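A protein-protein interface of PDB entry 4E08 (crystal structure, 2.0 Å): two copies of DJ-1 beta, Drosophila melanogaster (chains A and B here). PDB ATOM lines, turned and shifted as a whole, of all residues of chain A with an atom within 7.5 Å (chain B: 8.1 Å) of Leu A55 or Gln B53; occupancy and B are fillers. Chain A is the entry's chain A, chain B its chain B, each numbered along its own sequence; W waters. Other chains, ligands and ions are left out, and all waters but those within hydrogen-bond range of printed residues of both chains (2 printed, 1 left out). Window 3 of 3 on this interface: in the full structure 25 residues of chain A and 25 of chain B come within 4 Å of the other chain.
Among the printed residues, merely in contact across the chains: Ile A22 with Val B52 (3.3 Å), Ile A22 with Ile B22 (3.4 Å), Gln A53 with Ile B54 (3.5 Å), Ile A54 with Gln B53 (3.5 Å), Leu A55 with Leu B55 (3.6 Å), Ile A22 with Glu B18 (3.6 Å), Val A52 with Ile B54 (3.8 Å), Arg A29 with Asp B51 (3.8 Å), Arg A29 with Val B52 (3.8 Å), Ile A54 with Val B52 (3.8 Å), Ile A54 with Ile B22 (3.9 Å) and Ala A45 with Leu B55 (3.9 Å).
NH2 of Arg A29 lies within salt-bridge range of OD2 of Asp A57 (2.8 Å). N of Val A46 is in hydrogen-bond range of O of Ile A54, 2.8 Å away. OG of Ser B49 is in hydrogen-bond range of OE2 of Glu B18 (2.6 Å). OE1 of Glu B18 lies within hydrogen-bond range of N of Arg B50. O of Ile B54 lies within hydrogen-bond range of N of Val B46 (2.8 Å). The side-chain sulfur of Cys B48 lies close to the backbone carbonyl oxygen of Val B52 (3.8 Å).
Of chain B, only Gln B53 (2.9 Å) and Leu B55 (3.6 Å) come within 4 Å of Leu A55. Gln B53 touches two residues of chain A. Printed residues of chain B within 4 Å of Ile A22: Glu B18, Ile B22 and Val B52. Of the printed residues of chain A, Val B52 touches Ile A22, Arg A29 and Ile A54. Phe A21 touches none of the printed residues of chain B. The nearest residue of chain B that does not touch Leu A55 is Ala B45 (4.1 Å).
NH1 of Arg A29 lies within hydrogen-bond range of O of Arg B50, 2.9 Å away. The backbone NH (N) of Leu B55 sits at hydrogen-bond distance from the backbone carbonyl oxygen (O) of Gln A53 (3.0 Å). The backbone NH (N) of Leu A55 is in hydrogen-bond range of the backbone carbonyl oxygen (O) of Gln B53.
Water W1 bridges the backbone carbonyl oxygen of Leu A55 (2.5 Å) and the backbone NH of Gln B53 (2.5 Å). Water W2 lies within hydrogen-bond range of NH1 of Arg A29 (2.8 Å), OD1 of Asp A57 (2.8 Å) and O of Asp B51 (2.8 Å).
Of the 17 printed residues of chain A, 7 touch a printed residue of chain B. Hydrophobic or aromatic side chains of chain A that line the printed part of chain B: Ile A22, Ala A45, Val A52, Ile A54 and Leu A55. Of the 16 printed residues of chain B, 8 touch a printed residue of chain A. Among the printed residues, 15 pairs touch across the chains.
Ile A22 touches its own counterpart, Ile B22. Ile A22 touches Val B52, but with the chains exchanged Val A52 does not touch Ile B22 (4.3 Å). Gln A53 touches Ile B54, and with the chains exchanged Ile A54 touches Gln B53. Ile A54 touches Ile B22, but with the chains exchanged Ile A22 does not touch Ile B54 (5.1 Å). Of the 15 pairs that touch across the chains among the printed residues, 8 have their exchanged pair printed and touching as well.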
ATOM      1  N   LEU A  12       1.030  29.154 -29.559  1.00  0.00           N
ATOM      2  CA  LEU A  12      -0.324  29.599 -29.250  1.00  0.00           C
ATOM      3  C   LEU A  12      -0.316  31.093 -28.946  1.00  0.00           C
ATOM      4  O   LEU A  12       0.194  31.537 -27.922  1.00  0.00           O
ATOM      5  CB  LEU A  12      -0.903  28.761 -28.087  1.00  0.00           C
ATOM      6  CG  LEU A  12      -2.283  29.119 -27.520  1.00  0.00           C
ATOM      7  CD1 LEU A  12      -3.376  29.038 -28.602  1.00  0.00           C
ATOM      8  CD2 LEU A  12      -2.581  28.195 -26.289  1.00  0.00           C
ATOM      9  N   PHE A  21      -5.621  25.661 -34.483  1.00  0.00           N
ATOM     10  CA  PHE A  21      -4.723  25.300 -33.379  1.00  0.00           C
ATOM     11  C   PHE A  21      -5.004  23.901 -32.802  1.00  0.00           C
ATOM     12  O   PHE A  21      -4.076  23.093 -32.657  1.00  0.00           O
ATOM     13  CB  PHE A  21      -4.794  26.308 -32.200  1.00  0.00           C
ATOM     14  CG  PHE A  21      -4.196  25.737 -30.937  1.00  0.00           C
ATOM     15  CD1 PHE A  21      -2.809  25.574 -30.828  1.00  0.00           C
ATOM     16  CD2 PHE A  21      -5.012  25.255 -29.905  1.00  0.00           C
ATOM     17  CE1 PHE A  21      -2.238  24.986 -29.677  1.00  0.00           C
ATOM     18  CE2 PHE A  21      -4.452  24.675 -28.734  1.00  0.00           C
ATOM     19  CZ  PHE A  21      -3.053  24.541 -28.645  1.00  0.00           C
ATOM     20  N   ILE A  22      -6.267  23.662 -32.427  1.00  0.00           N
ATOM     21  CA  ILE A  22      -6.643  22.454 -31.676  1.00  0.00           C
ATOM     22  C   ILE A  22      -6.485  21.226 -32.589  1.00  0.00           C
ATOM     23  O   ILE A  22      -5.986  20.184 -32.167  1.00  0.00           O
ATOM     24  CB  ILE A  22      -8.068  22.574 -31.034  1.00  0.00           C
ATOM     25  CG1 ILE A  22      -8.254  21.588 -29.909  1.00  0.00           C
ATOM     26  CG2 ILE A  22      -9.214  22.290 -32.038  1.00  0.00           C
ATOM     27  CD1 ILE A  22      -7.210  21.809 -28.780  1.00  0.00           C
ATOM     28  N   ARG A  29      -0.619  14.769 -31.780  1.00  0.00           N
ATOM     29  CA  ARG A  29      -0.575  13.872 -30.624  1.00  0.00           C
ATOM     30  C   ARG A  29      -1.112  12.490 -30.953  1.00  0.00           C
ATOM     31  O   ARG A  29      -0.520  11.492 -30.530  1.00  0.00           O
ATOM     32  CB  ARG A  29      -1.296  14.493 -29.408  1.00  0.00           C
ATOM     33  CG  ARG A  29      -0.507  15.668 -28.800  1.00  0.00           C
ATOM     34  CD  ARG A  29      -1.020  16.183 -27.438  1.00  0.00           C
ATOM     35  NE  ARG A  29      -0.038  17.114 -26.845  1.00  0.00           N
ATOM     36  CZ  ARG A  29      -0.334  18.188 -26.119  1.00  0.00           C
ATOM     37  NH1 ARG A  29      -1.598  18.492 -25.870  1.00  0.00           N
ATOM     38  NH2 ARG A  29       0.640  18.990 -25.671  1.00  0.00           N
ATOM     39  N   VAL A  37       2.846  22.818 -26.613  1.00  0.00           N
ATOM     40  CA  VAL A  37       2.059  23.997 -26.887  1.00  0.00           C
ATOM     41  C   VAL A  37       2.723  25.125 -26.088  1.00  0.00           C
ATOM     42  O   VAL A  37       2.784  25.071 -24.857  1.00  0.00           O
ATOM     43  CB  VAL A  37       0.573  23.826 -26.493  1.00  0.00           C
ATOM     44  CG1 VAL A  37      -0.203  25.177 -26.640  1.00  0.00           C
ATOM     45  CG2 VAL A  37      -0.091  22.699 -27.309  1.00  0.00           C
ATOM     46  N   GLY A  39       2.823  29.077 -25.267  1.00  0.00           N
ATOM     47  CA  GLY A  39       2.144  30.373 -25.289  1.00  0.00           C
ATOM     48  C   GLY A  39       3.063  31.481 -25.758  1.00  0.00           C
ATOM     49  O   GLY A  39       4.206  31.568 -25.313  1.00  0.00           O
ATOM     50  N   GLY A  43       3.092  31.714 -19.900  1.00  0.00           N
ATOM     51  CA  GLY A  43       2.431  30.447 -19.622  1.00  0.00           C
ATOM     52  C   GLY A  43       0.941  30.572 -19.302  1.00  0.00           C
ATOM     53  O   GLY A  43       0.264  29.564 -19.006  1.00  0.00           O
ATOM     54  N   GLU A  44       0.431  31.799 -19.381  1.00  0.00           N
ATOM     55  CA  GLU A  44      -0.981  32.080 -19.059  1.00  0.00           C
ATOM     56  C   GLU A  44      -1.962  31.630 -20.165  1.00  0.00           C
ATOM     57  O   GLU A  44      -1.586  31.405 -21.326  1.00  0.00           O
ATOM     58  CB  GLU A  44      -1.198  33.566 -18.696  1.00  0.00           C
ATOM     59  CG  GLU A  44      -0.267  34.127 -17.581  1.00  0.00           C
ATOM     60  CD  GLU A  44      -0.477  33.485 -16.199  1.00  0.00           C
ATOM     61  OE1 GLU A  44       0.334  33.778 -15.285  1.00  0.00           O
ATOM     62  OE2 GLU A  44      -1.446  32.705 -16.012  1.00  0.00           O
ATOM     63  N   ALA A  45      -3.214  31.477 -19.781  1.00  0.00           N
ATOM     64  CA  ALA A  45      -4.287  31.107 -20.728  1.00  0.00           C
ATOM     65  C   ALA A  45      -4.320  32.095 -21.888  1.00  0.00           C
ATOM     66  O   ALA A  45      -4.168  33.309 -21.674  1.00  0.00           O
ATOM     67  CB  ALA A  45      -5.648  31.093 -20.002  1.00  0.00           C
ATOM     68  N   VAL A  46      -4.520  31.579 -23.101  1.00  0.00           N
ATOM     69  CA  VAL A  46      -4.540  32.418 -24.311  1.00  0.00           C
ATOM     70  C   VAL A  46      -5.980  32.523 -24.795  1.00  0.00           C
ATOM     71  O   VAL A  46      -6.655  31.521 -24.914  1.00  0.00           O
ATOM     72  CB  VAL A  46      -3.670  31.815 -25.388  1.00  0.00           C
ATOM     73  CG1 VAL A  46      -3.762  32.633 -26.682  1.00  0.00           C
ATOM     74  CG2 VAL A  46      -2.180  31.685 -24.883  1.00  0.00           C
ATOM     75  N   VAL A  52     -12.507  31.444 -26.992  1.00  0.00           N
ATOM     76  CA  VAL A  52     -12.141  30.231 -26.254  1.00  0.00           C
ATOM     77  C   VAL A  52     -10.751  30.466 -25.672  1.00  0.00           C
ATOM     78  O   VAL A  52      -9.818  30.895 -26.402  1.00  0.00           O
ATOM     79  CB  VAL A  52     -12.074  28.958 -27.183  1.00  0.00           C
ATOM     80  CG1 VAL A  52     -11.513  27.723 -26.434  1.00  0.00           C
ATOM     81  CG2 VAL A  52     -13.456  28.614 -27.747  1.00  0.00           C
ATOM     82  N   GLN A  53     -10.623  30.192 -24.372  1.00  0.00           N
ATOM     83  CA  GLN A  53      -9.357  30.331 -23.632  1.00  0.00           C
ATOM     84  C   GLN A  53      -8.658  29.015 -23.399  1.00  0.00           C
ATOM     85  O   GLN A  53      -9.256  28.042 -22.956  1.00  0.00           O
ATOM     86  CB  GLN A  53      -9.575  31.046 -22.304  1.00  0.00           C
ATOM     87  CG  GLN A  53      -9.975  32.494 -22.509  1.00  0.00           C
ATOM     88  CD  GLN A  53      -9.701  33.296 -21.308  1.00  0.00           C
ATOM     89  OE1 GLN A  53      -8.586  33.314 -20.817  1.00  0.00           O
ATOM     90  NE2 GLN A  53     -10.710  33.989 -20.819  1.00  0.00           N
ATOM     91  N   ILE A  54      -7.394  28.978 -23.736  1.00  0.00           N
ATOM     92  CA  ILE A  54      -6.682  27.699 -23.759  1.00  0.00           C
ATOM     93  C   ILE A  54      -5.421  27.855 -22.954  1.00  0.00           C
ATOM     94  O   ILE A  54      -4.686  28.818 -23.138  1.00  0.00           O
ATOM     95  CB  ILE A  54      -6.359  27.267 -25.216  1.00  0.00           C
ATOM     96  CG1 ILE A  54      -7.660  27.119 -26.020  1.00  0.00           C
ATOM     97  CG2 ILE A  54      -5.554  25.927 -25.262  1.00  0.00           C
ATOM     98  CD1 ILE A  54      -7.441  26.670 -27.456  1.00  0.00           C
ATOM     99  N   LEU A  55      -5.169  26.911 -22.059  1.00  0.00           N
ATOM    100  CA  LEU A  55      -3.903  26.861 -21.323  1.00  0.00           C
ATOM    101  C   LEU A  55      -2.805  26.254 -22.148  1.00  0.00           C
ATOM    102  O   LEU A  55      -2.918  25.099 -22.550  1.00  0.00           O
ATOM    103  CB  LEU A  55      -4.028  25.959 -20.112  1.00  0.00           C
ATOM    104  CG  LEU A  55      -4.297  26.580 -18.766  1.00  0.00           C
ATOM    105  CD1 LEU A  55      -5.764  26.920 -18.659  1.00  0.00           C
ATOM    106  CD2 LEU A  55      -3.888  25.563 -17.683  1.00  0.00           C
ATOM    107  N   PRO A  56      -1.709  27.004 -22.359  1.00  0.00           N
ATOM    108  CA  PRO A  56      -0.546  26.402 -22.991  1.00  0.00           C
ATOM    109  C   PRO A  56       0.165  25.429 -22.047  1.00  0.00           C
ATOM    110  O   PRO A  56      -0.074  25.464 -20.826  1.00  0.00           O
ATOM    111  CB  PRO A  56       0.333  27.611 -23.292  1.00  0.00           C
ATOM    112  CG  PRO A  56       0.062  28.550 -22.171  1.00  0.00           C
ATOM    113  CD  PRO A  56      -1.432  28.378 -21.886  1.00  0.00           C
ATOM    114  N   ASP A  57       1.030  24.573 -22.596  1.00  0.00           N
ATOM    115  CA  ASP A  57       1.835  23.660 -21.781  1.00  0.00           C
ATOM    116  C   ASP A  57       2.928  24.464 -21.049  1.00  0.00           C
ATOM    117  O   ASP A  57       3.273  24.193 -19.898  1.00  0.00           O
ATOM    118  CB  ASP A  57       2.505  22.592 -22.661  1.00  0.00           C
ATOM    119  CG  ASP A  57       1.518  21.659 -23.322  1.00  0.00           C
ATOM    120  OD1 ASP A  57       0.513  21.329 -22.709  1.00  0.00           O
ATOM    121  OD2 ASP A  57       1.744  21.245 -24.475  1.00  0.00           O
ATOM    122  N   THR A  58       3.479  25.453 -21.746  1.00  0.00           N
ATOM    123  CA  THR A  58       4.565  26.284 -21.243  1.00  0.00           C
ATOM    124  C   THR A  58       4.622  27.578 -22.085  1.00  0.00           C
ATOM    125  O   THR A  58       3.749  27.801 -22.936  1.00  0.00           O
ATOM    126  CB  THR A  58       5.913  25.490 -21.293  1.00  0.00           C
ATOM    127  OG1 THR A  58       6.934  26.286 -20.715  1.00  0.00           O
ATOM    128  CG2 THR A  58       6.293  25.161 -22.772  1.00  0.00           C
ATOM    129  N   LEU B  12     -18.748  21.370 -21.582  1.00  0.00           N
ATOM    130  CA  LEU B  12     -17.358  20.918 -21.666  1.00  0.00           C
ATOM    131  C   LEU B  12     -17.002  20.015 -20.492  1.00  0.00           C
ATOM    132  O   LEU B  12     -16.991  20.455 -19.334  1.00  0.00           O
ATOM    133  CB  LEU B  12     -16.418  22.134 -21.750  1.00  0.00           C
ATOM    134  CG  LEU B  12     -14.881  21.928 -21.711  1.00  0.00           C
ATOM    135  CD1 LEU B  12     -14.368  21.102 -22.982  1.00  0.00           C
ATOM    136  CD2 LEU B  12     -14.209  23.279 -21.631  1.00  0.00           C
ATOM    137  N   GLU B  18     -11.449  17.447 -27.819  1.00  0.00           N
ATOM    138  CA  GLU B  18     -11.331  18.919 -27.870  1.00  0.00           C
ATOM    139  C   GLU B  18     -11.629  19.530 -29.234  1.00  0.00           C
ATOM    140  O   GLU B  18     -12.030  20.693 -29.326  1.00  0.00           O
ATOM    141  CB  GLU B  18      -9.972  19.405 -27.341  1.00  0.00           C
ATOM    142  CG  GLU B  18      -8.751  18.620 -27.850  1.00  0.00           C
ATOM    143  CD  GLU B  18      -8.473  17.407 -26.966  1.00  0.00           C
ATOM    144  OE1 GLU B  18      -7.555  17.455 -26.142  1.00  0.00           O
ATOM    145  OE2 GLU B  18      -9.237  16.420 -27.075  1.00  0.00           O
ATOM    146  N   ILE B  22     -14.195  22.447 -29.783  1.00  0.00           N
ATOM    147  CA  ILE B  22     -13.810  23.784 -30.237  1.00  0.00           C
ATOM    148  C   ILE B  22     -14.585  24.136 -31.529  1.00  0.00           C
ATOM    149  O   ILE B  22     -15.080  25.244 -31.688  1.00  0.00           O
ATOM    150  CB  ILE B  22     -12.280  23.954 -30.381  1.00  0.00           C
ATOM    151  CG1 ILE B  22     -11.697  24.291 -28.998  1.00  0.00           C
ATOM    152  CG2 ILE B  22     -11.925  25.194 -31.172  1.00  0.00           C
ATOM    153  CD1 ILE B  22     -10.109  24.263 -28.885  1.00  0.00           C
ATOM    154  N   GLU B  44     -13.700  25.625 -13.476  1.00  0.00           N
ATOM    155  CA  GLU B  44     -12.222  25.503 -13.616  1.00  0.00           C
ATOM    156  C   GLU B  44     -11.803  24.860 -14.954  1.00  0.00           C
ATOM    157  O   GLU B  44     -12.651  24.315 -15.670  1.00  0.00           O
ATOM    158  CB  GLU B  44     -11.638  24.773 -12.405  1.00  0.00           C
ATOM    159  CG  GLU B  44     -11.625  25.635 -11.098  1.00  0.00           C
ATOM    160  CD  GLU B  44     -11.125  24.874  -9.859  1.00  0.00           C
ATOM    161  OE1 GLU B  44     -11.373  23.648  -9.752  1.00  0.00           O
ATOM    162  OE2 GLU B  44     -10.491  25.496  -8.969  1.00  0.00           O
ATOM    163  N   ALA B  45     -10.517  24.953 -15.314  1.00  0.00           N
ATOM    164  CA  ALA B  45     -10.072  24.447 -16.612  1.00  0.00           C
ATOM    165  C   ALA B  45     -10.452  22.991 -16.758  1.00  0.00           C
ATOM    166  O   ALA B  45     -10.514  22.279 -15.784  1.00  0.00           O
ATOM    167  CB  ALA B  45      -8.562  24.634 -16.800  1.00  0.00           C
ATOM    168  N   VAL B  46     -10.739  22.559 -17.978  1.00  0.00           N
ATOM    169  CA  VAL B  46     -11.140  21.175 -18.214  1.00  0.00           C
ATOM    170  C   VAL B  46     -10.014  20.542 -19.035  1.00  0.00           C
ATOM    171  O   VAL B  46      -9.661  21.052 -20.126  1.00  0.00           O
ATOM    172  CB  VAL B  46     -12.513  21.093 -18.969  1.00  0.00           C
ATOM    173  CG1 VAL B  46     -12.913  19.627 -19.355  1.00  0.00           C
ATOM    174  CG2 VAL B  46     -13.631  21.780 -18.170  1.00  0.00           C
ATOM    175  N   LYS B  47      -9.422  19.474 -18.503  1.00  0.00           N
ATOM    176  CA  LYS B  47      -8.450  18.702 -19.285  1.00  0.00           C
ATOM    177  C   LYS B  47      -9.160  17.793 -20.303  1.00  0.00           C
ATOM    178  O   LYS B  47      -9.993  16.969 -19.913  1.00  0.00           O
ATOM    179  CB  LYS B  47      -7.527  17.871 -18.387  1.00  0.00           C
ATOM    180  CG  LYS B  47      -6.366  17.266 -19.160  1.00  0.00           C
ATOM    181  CD  LYS B  47      -5.187  16.867 -18.287  1.00  0.00           C
ATOM    182  CE  LYS B  47      -5.175  15.410 -17.967  1.00  0.00           C
ATOM    183  NZ  LYS B  47      -3.907  15.043 -17.201  1.00  0.00           N
ATOM    184  N   CYS B  48      -8.818  17.939 -21.590  1.00  0.00           N
ATOM    185  CA  CYS B  48      -9.489  17.187 -22.681  1.00  0.00           C
ATOM    186  C   CYS B  48      -8.728  15.887 -23.092  1.00  0.00           C
ATOM    187  O   CYS B  48      -7.623  15.632 -22.623  1.00  0.00           O
ATOM    188  CB  CYS B  48      -9.729  18.105 -23.907  1.00  0.00           C
ATOM    189  SG  CYS B  48     -10.942  19.416 -23.615  1.00  0.00           S
ATOM    190  N   SER B  49      -9.311  15.104 -24.005  1.00  0.00           N
ATOM    191  CA  SER B  49      -8.793  13.773 -24.387  1.00  0.00           C
ATOM    192  C   SER B  49      -7.323  13.733 -24.783  1.00  0.00           C
ATOM    193  O   SER B  49      -6.656  12.721 -24.618  1.00  0.00           O
ATOM    194  CB  SER B  49      -9.642  13.148 -25.511  1.00  0.00           C
ATOM    195  OG  SER B  49      -9.445  13.798 -26.762  1.00  0.00           O
ATOM    196  N   ARG B  50      -6.821  14.815 -25.347  1.00  0.00           N
ATOM    197  CA  ARG B  50      -5.441  14.842 -25.795  1.00  0.00           C
ATOM    198  C   ARG B  50      -4.625  15.880 -25.022  1.00  0.00           C
ATOM    199  O   ARG B  50      -3.650  16.439 -25.545  1.00  0.00           O
ATOM    200  CB  ARG B  50      -5.352  15.063 -27.312  1.00  0.00           C
ATOM    201  CG  ARG B  50      -6.059  14.031 -28.159  1.00  0.00           C
ATOM    202  CD  ARG B  50      -5.543  12.624 -28.009  1.00  0.00           C
ATOM    203  NE  ARG B  50      -6.570  11.714 -28.503  1.00  0.00           N
ATOM    204  CZ  ARG B  50      -6.342  10.502 -28.989  1.00  0.00           C
ATOM    205  NH1 ARG B  50      -5.085  10.018 -29.070  1.00  0.00           N
ATOM    206  NH2 ARG B  50      -7.392   9.780 -29.393  1.00  0.00           N
ATOM    207  N   ASP B  51      -5.027  16.093 -23.760  1.00  0.00           N
ATOM    208  CA  ASP B  51      -4.311  16.932 -22.797  1.00  0.00           C
ATOM    209  C   ASP B  51      -4.327  18.440 -23.084  1.00  0.00           C
ATOM    210  O   ASP B  51      -3.468  19.164 -22.620  1.00  0.00           O
ATOM    211  CB  ASP B  51      -2.854  16.464 -22.649  1.00  0.00           C
ATOM    212  CG  ASP B  51      -2.744  15.093 -22.047  1.00  0.00           C
ATOM    213  OD1 ASP B  51      -3.691  14.625 -21.384  1.00  0.00           O
ATOM    214  OD2 ASP B  51      -1.691  14.474 -22.231  1.00  0.00           O
ATOM    215  N   VAL B  52      -5.265  18.901 -23.886  1.00  0.00           N
ATOM    216  CA  VAL B  52      -5.424  20.329 -24.063  1.00  0.00           C
ATOM    217  C   VAL B  52      -6.365  20.813 -22.936  1.00  0.00           C
ATOM    218  O   VAL B  52      -7.372  20.170 -22.625  1.00  0.00           O
ATOM    219  CB  VAL B  52      -5.980  20.644 -25.458  1.00  0.00           C
ATOM    220  CG1 VAL B  52      -6.132  22.145 -25.636  1.00  0.00           C
ATOM    221  CG2 VAL B  52      -5.021  20.049 -26.554  1.00  0.00           C
ATOM    222  N   GLN B  53      -6.031  21.934 -22.329  1.00  0.00           N
ATOM    223  CA  GLN B  53      -6.793  22.399 -21.198  1.00  0.00           C
ATOM    224  C   GLN B  53      -7.529  23.672 -21.562  1.00  0.00           C
ATOM    225  O   GLN B  53      -6.907  24.640 -22.001  1.00  0.00           O
ATOM    226  CB  GLN B  53      -5.875  22.549 -19.966  1.00  0.00           C
ATOM    227  CG  GLN B  53      -5.560  21.176 -19.379  1.00  0.00           C
ATOM    228  CD  GLN B  53      -4.815  21.225 -18.067  1.00  0.00           C
ATOM    229  OE1 GLN B  53      -5.095  22.063 -17.210  1.00  0.00           O
ATOM    230  NE2 GLN B  53      -3.852  20.315 -17.897  1.00  0.00           N
ATOM    231  N   ILE B  54      -8.848  23.648 -21.392  1.00  0.00           N
ATOM    232  CA  ILE B  54      -9.740  24.745 -21.821  1.00  0.00           C
ATOM    233  C   ILE B  54     -10.542  25.343 -20.655  1.00  0.00           C
ATOM    234  O   ILE B  54     -11.162  24.617 -19.877  1.00  0.00           O
ATOM    235  CB  ILE B  54     -10.670  24.278 -22.973  1.00  0.00           C
ATOM    236  CG1 ILE B  54      -9.820  23.702 -24.108  1.00  0.00           C
ATOM    237  CG2 ILE B  54     -11.634  25.419 -23.438  1.00  0.00           C
ATOM    238  CD1 ILE B  54     -10.647  23.093 -25.240  1.00  0.00           C
ATOM    239  N   LEU B  55     -10.511  26.671 -20.546  1.00  0.00           N
ATOM    240  CA  LEU B  55     -11.270  27.383 -19.532  1.00  0.00           C
ATOM    241  C   LEU B  55     -12.676  27.542 -20.010  1.00  0.00           C
ATOM    242  O   LEU B  55     -12.914  28.081 -21.103  1.00  0.00           O
ATOM    243  CB  LEU B  55     -10.703  28.778 -19.233  1.00  0.00           C
ATOM    244  CG  LEU B  55      -9.280  28.940 -18.711  1.00  0.00           C
ATOM    245  CD1 LEU B  55      -9.019  30.370 -18.183  1.00  0.00           C
ATOM    246  CD2 LEU B  55      -9.051  27.948 -17.596  1.00  0.00           C
ATOM    247  N   PRO B  56     -13.641  27.055 -19.211  1.00  0.00           N
ATOM    248  CA  PRO B  56     -15.054  27.281 -19.571  1.00  0.00           C
ATOM    249  C   PRO B  56     -15.466  28.724 -19.318  1.00  0.00           C
ATOM    250  O   PRO B  56     -14.782  29.430 -18.591  1.00  0.00           O
ATOM    251  CB  PRO B  56     -15.816  26.349 -18.617  1.00  0.00           C
ATOM    252  CG  PRO B  56     -14.907  26.108 -17.493  1.00  0.00           C
ATOM    253  CD  PRO B  56     -13.476  26.271 -17.984  1.00  0.00           C
HETATM  254  O   HOH W   1      -3.610  22.725 -22.371  1.00  0.00           O
HETATM  255  O   HOH W   2      -1.757  20.729 -24.225  1.00  0.00           O
